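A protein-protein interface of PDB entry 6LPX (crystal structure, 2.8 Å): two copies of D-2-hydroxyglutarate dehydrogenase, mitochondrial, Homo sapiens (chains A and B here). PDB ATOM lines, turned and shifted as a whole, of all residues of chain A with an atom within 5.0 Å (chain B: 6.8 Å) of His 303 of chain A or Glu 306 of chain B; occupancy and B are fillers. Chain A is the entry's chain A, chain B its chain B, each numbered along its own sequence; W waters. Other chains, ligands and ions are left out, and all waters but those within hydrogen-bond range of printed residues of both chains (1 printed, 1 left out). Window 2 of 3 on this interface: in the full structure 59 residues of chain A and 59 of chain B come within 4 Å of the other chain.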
ATOM      1  N   ASN A 300      -6.471  14.396 -24.914  1.00  0.00           N
ATOM      2  CA  ASN A 300      -7.232  14.765 -23.727  1.00  0.00           C
ATOM      3  C   ASN A 300      -6.265  14.866 -22.556  1.00  0.00           C
ATOM      4  O   ASN A 300      -5.808  13.846 -22.030  1.00  0.00           O
ATOM      5  CB  ASN A 300      -8.319  13.727 -23.471  1.00  0.00           C
ATOM      6  CG  ASN A 300      -9.253  14.120 -22.378  1.00  0.00           C
ATOM      7  OD1 ASN A 300      -8.836  14.503 -21.289  1.00  0.00           O
ATOM      8  ND2 ASN A 300     -10.547  13.991 -22.647  1.00  0.00           N
ATOM      9  N   ALA A 301      -5.985  16.097 -22.129  1.00  0.00           N
ATOM     10  CA  ALA A 301      -4.990  16.320 -21.079  1.00  0.00           C
ATOM     11  C   ALA A 301      -5.367  15.630 -19.771  1.00  0.00           C
ATOM     12  O   ALA A 301      -4.491  15.142 -19.047  1.00  0.00           O
ATOM     13  CB  ALA A 301      -4.791  17.819 -20.862  1.00  0.00           C
ATOM     14  N   GLY A 302      -6.658  15.574 -19.444  1.00  0.00           N
ATOM     15  CA  GLY A 302      -7.060  14.925 -18.204  1.00  0.00           C
ATOM     16  C   GLY A 302      -6.865  13.421 -18.213  1.00  0.00           C
ATOM     17  O   GLY A 302      -6.419  12.840 -17.216  1.00  0.00           O
ATOM     18  N   HIS A 303      -7.203  12.762 -19.331  1.00  0.00           N
ATOM     19  CA  HIS A 303      -6.961  11.322 -19.434  1.00  0.00           C
ATOM     20  C   HIS A 303      -5.475  10.999 -19.359  1.00  0.00           C
ATOM     21  O   HIS A 303      -5.071  10.037 -18.692  1.00  0.00           O
ATOM     22  CB  HIS A 303      -7.576  10.762 -20.717  1.00  0.00           C
ATOM     23  CG  HIS A 303      -9.071  10.768 -20.719  1.00  0.00           C
ATOM     24  ND1 HIS A 303      -9.817  10.911 -21.869  1.00  0.00           N
ATOM     25  CD2 HIS A 303      -9.962  10.616 -19.713  1.00  0.00           C
ATOM     26  CE1 HIS A 303     -11.101  10.872 -21.567  1.00  0.00           C
ATOM     27  NE2 HIS A 303     -11.216  10.689 -20.265  1.00  0.00           N
ATOM     28  N   ASP A 304      -4.651  11.787 -20.049  1.00  0.00           N
ATOM     29  CA  ASP A 304      -3.212  11.594 -19.983  1.00  0.00           C
ATOM     30  C   ASP A 304      -2.711  11.756 -18.559  1.00  0.00           C
ATOM     31  O   ASP A 304      -1.947  10.921 -18.060  1.00  0.00           O
ATOM     32  CB  ASP A 304      -2.505  12.560 -20.931  1.00  0.00           C
ATOM     33  CG  ASP A 304      -2.814  12.275 -22.398  1.00  0.00           C
ATOM     34  OD1 ASP A 304      -3.673  11.409 -22.708  1.00  0.00           O
ATOM     35  OD2 ASP A 304      -2.130  12.880 -23.249  1.00  0.00           O
ATOM     36  N   ALA A 305      -3.123  12.835 -17.892  1.00  0.00           N
ATOM     37  CA  ALA A 305      -2.696  13.067 -16.516  1.00  0.00           C
ATOM     38  C   ALA A 305      -3.106  11.919 -15.592  1.00  0.00           C
ATOM     39  O   ALA A 305      -2.319  11.491 -14.737  1.00  0.00           O
ATOM     40  CB  ALA A 305      -3.269  14.390 -16.013  1.00  0.00           C
ATOM     41  N   GLU A 306      -4.318  11.377 -15.776  1.00  0.00           N
ATOM     42  CA  GLU A 306      -4.744  10.230 -14.977  1.00  0.00           C
ATOM     43  C   GLU A 306      -3.880   8.996 -15.243  1.00  0.00           C
ATOM     44  O   GLU A 306      -3.487   8.280 -14.302  1.00  0.00           O
ATOM     45  CB  GLU A 306      -6.218   9.952 -15.255  1.00  0.00           C
ATOM     46  CG  GLU A 306      -7.105  11.032 -14.615  1.00  0.00           C
ATOM     47  CD  GLU A 306      -8.617  10.815 -14.754  1.00  0.00           C
ATOM     48  OE1 GLU A 306      -9.051  10.006 -15.602  1.00  0.00           O
ATOM     49  OE2 GLU A 306      -9.384  11.481 -14.015  1.00  0.00           O
ATOM     50  N   LYS A 307      -3.561   8.738 -16.519  1.00  0.00           N
ATOM     51  CA  LYS A 307      -2.706   7.607 -16.848  1.00  0.00           C
ATOM     52  C   LYS A 307      -1.326   7.767 -16.209  1.00  0.00           C
ATOM     53  O   LYS A 307      -0.793   6.823 -15.612  1.00  0.00           O
ATOM     54  CB  LYS A 307      -2.557   7.402 -18.355  1.00  0.00           C
ATOM     55  CG  LYS A 307      -3.781   6.757 -19.045  1.00  0.00           C
ATOM     56  CD  LYS A 307      -3.450   6.469 -20.499  1.00  0.00           C
ATOM     57  CE  LYS A 307      -4.477   5.670 -21.328  1.00  0.00           C
ATOM     58  NZ  LYS A 307      -5.590   6.465 -21.956  1.00  0.00           N
ATOM     59  N   MET B 256     -11.657  14.830 -31.264  1.00  0.00           N
ATOM     60  CA  MET B 256     -12.116  14.387 -29.956  1.00  0.00           C
ATOM     61  C   MET B 256     -11.657  12.996 -29.563  1.00  0.00           C
ATOM     62  O   MET B 256     -11.482  12.732 -28.370  1.00  0.00           O
ATOM     63  CB  MET B 256     -13.641  14.452 -29.908  1.00  0.00           C
ATOM     64  CG  MET B 256     -14.147  15.865 -30.062  1.00  0.00           C
ATOM     65  SD  MET B 256     -15.925  15.960 -29.883  1.00  0.00           S
ATOM     66  CE  MET B 256     -16.088  15.626 -28.135  1.00  0.00           C
ATOM     67  N   LEU B 257     -11.411  12.116 -30.527  1.00  0.00           N
ATOM     68  CA  LEU B 257     -10.908  10.792 -30.192  1.00  0.00           C
ATOM     69  C   LEU B 257      -9.398  10.738 -30.268  1.00  0.00           C
ATOM     70  O   LEU B 257      -8.764  10.072 -29.449  1.00  0.00           O
ATOM     71  CB  LEU B 257     -11.518   9.747 -31.130  1.00  0.00           C
ATOM     72  CG  LEU B 257     -13.045   9.768 -31.241  1.00  0.00           C
ATOM     73  CD1 LEU B 257     -13.516   8.658 -32.154  1.00  0.00           C
ATOM     74  CD2 LEU B 257     -13.693   9.663 -29.869  1.00  0.00           C
ATOM     75  N   GLU B 259      -5.633  10.073 -30.545  1.00  0.00           N
ATOM     76  CA  GLU B 259      -4.687   8.964 -30.656  1.00  0.00           C
ATOM     77  C   GLU B 259      -5.314   7.579 -30.519  1.00  0.00           C
ATOM     78  O   GLU B 259      -4.679   6.600 -30.918  1.00  0.00           O
ATOM     79  CB  GLU B 259      -3.572   9.136 -29.625  1.00  0.00           C
ATOM     80  CG  GLU B 259      -4.013   8.880 -28.202  1.00  0.00           C
ATOM     81  CD  GLU B 259      -4.850  10.005 -27.623  1.00  0.00           C
ATOM     82  OE1 GLU B 259      -5.565   9.753 -26.631  1.00  0.00           O
ATOM     83  OE2 GLU B 259      -4.810  11.127 -28.165  1.00  0.00           O
ATOM     84  N   ALA B 301     -10.016   1.311 -21.045  1.00  0.00           N
ATOM     85  CA  ALA B 301     -11.418   1.235 -21.460  1.00  0.00           C
ATOM     86  C   ALA B 301     -12.214   2.464 -21.036  1.00  0.00           C
ATOM     87  O   ALA B 301     -12.871   3.104 -21.863  1.00  0.00           O
ATOM     88  CB  ALA B 301     -12.067  -0.029 -20.885  1.00  0.00           C
ATOM     89  N   GLY B 302     -12.159   2.799 -19.742  1.00  0.00           N
ATOM     90  CA  GLY B 302     -12.847   3.974 -19.225  1.00  0.00           C
ATOM     91  C   GLY B 302     -12.549   5.267 -19.956  1.00  0.00           C
ATOM     92  O   GLY B 302     -13.464   6.020 -20.305  1.00  0.00           O
ATOM     93  N   HIS B 303     -11.265   5.546 -20.209  1.00  0.00           N
ATOM     94  CA  HIS B 303     -10.927   6.784 -20.907  1.00  0.00           C
ATOM     95  C   HIS B 303     -11.439   6.774 -22.336  1.00  0.00           C
ATOM     96  O   HIS B 303     -11.938   7.796 -22.826  1.00  0.00           O
ATOM     97  CB  HIS B 303      -9.423   7.047 -20.892  1.00  0.00           C
ATOM     98  CG  HIS B 303      -8.860   7.263 -19.526  1.00  0.00           C
ATOM     99  ND1 HIS B 303      -7.527   7.074 -19.230  1.00  0.00           N
ATOM    100  CD2 HIS B 303      -9.455   7.635 -18.370  1.00  0.00           C
ATOM    101  CE1 HIS B 303      -7.321   7.347 -17.955  1.00  0.00           C
ATOM    102  NE2 HIS B 303      -8.476   7.684 -17.409  1.00  0.00           N
ATOM    103  N   ASP B 304     -11.281   5.650 -23.033  1.00  0.00           N
ATOM    104  CA  ASP B 304     -11.781   5.563 -24.396  1.00  0.00           C
ATOM    105  C   ASP B 304     -13.286   5.737 -24.422  1.00  0.00           C
ATOM    106  O   ASP B 304     -13.823   6.413 -25.308  1.00  0.00           O
ATOM    107  CB  ASP B 304     -11.396   4.230 -25.020  1.00  0.00           C
ATOM    108  CG  ASP B 304      -9.911   4.097 -25.226  1.00  0.00           C
ATOM    109  OD1 ASP B 304      -9.165   4.977 -24.740  1.00  0.00           O
ATOM    110  OD2 ASP B 304      -9.496   3.105 -25.868  1.00  0.00           O
ATOM    111  N   ALA B 305     -13.980   5.163 -23.435  1.00  0.00           N
ATOM    112  CA  ALA B 305     -15.426   5.326 -23.345  1.00  0.00           C
ATOM    113  C   ALA B 305     -15.810   6.782 -23.152  1.00  0.00           C
ATOM    114  O   ALA B 305     -16.760   7.257 -23.778  1.00  0.00           O
ATOM    115  CB  ALA B 305     -15.987   4.473 -22.210  1.00  0.00           C
ATOM    116  N   GLU B 306     -15.094   7.506 -22.288  1.00  0.00           N
ATOM    117  CA  GLU B 306     -15.371   8.933 -22.124  1.00  0.00           C
ATOM    118  C   GLU B 306     -15.146   9.710 -23.421  1.00  0.00           C
ATOM    119  O   GLU B 306     -15.998  10.516 -23.833  1.00  0.00           O
ATOM    120  CB  GLU B 306     -14.489   9.532 -21.019  1.00  0.00           C
ATOM    121  CG  GLU B 306     -15.161   9.762 -19.667  1.00  0.00           C
ATOM    122  CD  GLU B 306     -14.233  10.420 -18.636  1.00  0.00           C
ATOM    123  OE1 GLU B 306     -13.749  11.548 -18.890  1.00  0.00           O
ATOM    124  OE2 GLU B 306     -13.984   9.814 -17.570  1.00  0.00           O
ATOM    125  N   LYS B 307     -14.013   9.471 -24.083  1.00  0.00           N
ATOM    126  CA  LYS B 307     -13.769  10.135 -25.363  1.00  0.00           C
ATOM    127  C   LYS B 307     -14.874   9.862 -26.369  1.00  0.00           C
ATOM    128  O   LYS B 307     -15.434  10.796 -26.954  1.00  0.00           O
ATOM    129  CB  LYS B 307     -12.431   9.689 -25.953  1.00  0.00           C
ATOM    130  CG  LYS B 307     -11.213  10.352 -25.381  1.00  0.00           C
ATOM    131  CD  LYS B 307      -9.996   9.989 -26.217  1.00  0.00           C
ATOM    132  CE  LYS B 307      -8.773  10.745 -25.746  1.00  0.00           C
ATOM    133  NZ  LYS B 307      -8.210  10.149 -24.512  1.00  0.00           N
ATOM    134  N   LEU B 308     -15.232   8.587 -26.545  1.00  0.00           N
ATOM    135  CA  LEU B 308     -16.269   8.233 -27.507  1.00  0.00           C
ATOM    136  C   LEU B 308     -17.629   8.803 -27.123  1.00  0.00           C
ATOM    137  O   LEU B 308     -18.346   9.315 -27.986  1.00  0.00           O
ATOM    138  CB  LEU B 308     -16.327   6.711 -27.682  1.00  0.00           C
ATOM    139  CG  LEU B 308     -16.970   6.265 -29.001  1.00  0.00           C
ATOM    140  CD1 LEU B 308     -16.189   6.799 -30.185  1.00  0.00           C
ATOM    141  CD2 LEU B 308     -17.102   4.756 -29.107  1.00  0.00           C
ATOM    142  N   GLY B 309     -18.010   8.711 -25.843  1.00  0.00           N
ATOM    143  CA  GLY B 309     -19.279   9.280 -25.402  1.00  0.00           C
ATOM    144  C   GLY B 309     -19.409  10.758 -25.712  1.00  0.00           C
ATOM    145  O   GLY B 309     -20.422  11.206 -26.263  1.00  0.00           O
ATOM    146  N   HIS B 310     -18.370  11.536 -25.387  1.00  0.00           N
ATOM    147  CA  HIS B 310     -18.423  12.964 -25.693  1.00  0.00           C
ATOM    148  C   HIS B 310     -18.445  13.186 -27.199  1.00  0.00           C
ATOM    149  O   HIS B 310     -19.181  14.053 -27.689  1.00  0.00           O
ATOM    150  CB  HIS B 310     -17.258  13.715 -25.037  1.00  0.00           C
ATOM    151  CG  HIS B 310     -17.448  15.207 -24.976  1.00  0.00           C
ATOM    152  ND1 HIS B 310     -18.693  15.806 -24.967  1.00  0.00           N
ATOM    153  CD2 HIS B 310     -16.549  16.218 -24.903  1.00  0.00           C
ATOM    154  CE1 HIS B 310     -18.554  17.119 -24.908  1.00  0.00           C
ATOM    155  NE2 HIS B 310     -17.262  17.396 -24.868  1.00  0.00           N
ATOM    156  N   PHE B 311     -17.668  12.399 -27.950  1.00  0.00           N
ATOM    157  CA  PHE B 311     -17.687  12.521 -29.404  1.00  0.00           C
ATOM    158  C   PHE B 311     -19.090  12.311 -29.961  1.00  0.00           C
ATOM    159  O   PHE B 311     -19.546  13.079 -30.812  1.00  0.00           O
ATOM    160  CB  PHE B 311     -16.718  11.528 -30.038  1.00  0.00           C
ATOM    161  CG  PHE B 311     -16.985  11.288 -31.490  1.00  0.00           C
ATOM    162  CD1 PHE B 311     -16.690  12.266 -32.427  1.00  0.00           C
ATOM    163  CD2 PHE B 311     -17.538  10.096 -31.923  1.00  0.00           C
ATOM    164  CE1 PHE B 311     -16.944  12.068 -33.762  1.00  0.00           C
ATOM    165  CE2 PHE B 311     -17.795   9.891 -33.260  1.00  0.00           C
ATOM    166  CZ  PHE B 311     -17.497  10.883 -34.180  1.00  0.00           C
ATOM    167  N   GLU B 313     -22.164  12.409 -28.355  1.00  0.00           N
ATOM    168  CA  GLU B 313     -22.966  13.555 -27.924  1.00  0.00           C
ATOM    169  C   GLU B 313     -22.776  14.764 -28.849  1.00  0.00           C
ATOM    170  O   GLU B 313     -23.748  15.313 -29.366  1.00  0.00           O
ATOM    171  CB  GLU B 313     -22.711  13.878 -26.433  1.00  0.00           C
ATOM    172  CG  GLU B 313     -21.830  15.080 -26.094  1.00  0.00           C
ATOM    173  CD  GLU B 313     -21.820  15.419 -24.602  1.00  0.00           C
ATOM    174  OE1 GLU B 313     -22.519  16.389 -24.215  1.00  0.00           O
ATOM    175  OE2 GLU B 313     -21.123  14.722 -23.822  1.00  0.00           O
HETATM  176  O   HOH W   1      -6.770   4.667 -23.445  1.00  0.00           O
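Water W1 lies within hydrogen-bond range of NZ of Lys 307 of chain A (2.6 Å) and OD1 of Asp 304 of chain B (2.7 Å).
His 303 of chain A touches its own counterpart, His 303 of chain B. His 303 of chain A touches Glu 306 of chain B, and with the chains exchanged Glu 306 of chain A touches His 303 of chain B. His 303 of chain A touches Lys 307 of chain B, and with the chains exchanged Lys 307 of chain A touches His 303 of chain B. Positions printed for both chains: 301, 302, 303, 304, 305, 306 and 307.
Among the printed residues, merely in contact across the chains: His 303 of chain A with His 303 of chain B (3.3 Å) and Asn 300 of chain A with Lys 307 of chain B (3.7 Å).
The backbone NH of Gly 302 of chain A lies within hydrogen-bond range of the side-chain amide oxygen of Asn 300 of chain A (3.0 Å). The backbone NH (N) of His 303 of chain A is in hydrogen-bond range of the side-chain amide oxygen (OD1) of Asn 300 of chain A, 3.1 Å away. OE1 of Glu 259 of chain B lies within salt-bridge range of NZ of Lys 307 of chain B, at 3.4 Å.
Printed residues of chain B within 4 Å of Asn 300 of chain A: Lys 307. Of chain B, only His 303 (3.3 Å), Glu 306 (3.0 Å) and Lys 307 (3.2 Å) come within 4 Å of His 303 of chain A. Printed residues of chain B within 4 Å of Glu 306 of chain A: His 303 (3.0 Å). Of the printed residues of chain B, Lys 307 of chain A touches His 303 (3.4 Å). Printed residues of chain A within 4 Å of Glu 306 of chain B: His 303. Printed residues of chain A within 4 Å of Lys 307 of chain B: Asn 300 and His 303. The nearest residue of chain B that does not touch His 303 of chain A is Gly 302 of chain B (5.2 Å). The nearest printed residue of chain B that does not touch Asn 300 of chain A is Glu 259 of chain B (4.9 Å).
The side-chain carboxylate of Glu 306 of chain B lies within hydrogen-bond range of a ring nitrogen (NE2) of His 303 of chain A, 3.0 Å away. ND1 of His 303 of chain A lies within hydrogen-bond range of NZ of Lys 307 of chain B (3.2 Å). The side-chain carboxylate of Glu 306 of chain A lies within hydrogen-bond range of a ring nitrogen (NE2) of His 303 of chain B (3.0 Å). ND1 of His 303 of chain B is in hydrogen-bond range of NZ of Lys 307 of chain A, at 3.4 Å.
Of the 15 printed residues of chain B, 3 touch a printed residue of chain A. Printed residues of chain B that touch a printed residue of chain A: His 303, Glu 306 and Lys 307. Hydrophobic or aromatic side chains of chain B within 4 Å of the printed part of chain A: His 303. Of the 8 printed residues of chain A, 4 touch a printed residue of chain B. Among the printed residues, no Asp or Glu carboxylate lies within 4 Å of a Lys or Arg side-chain nitrogen of the other chain.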
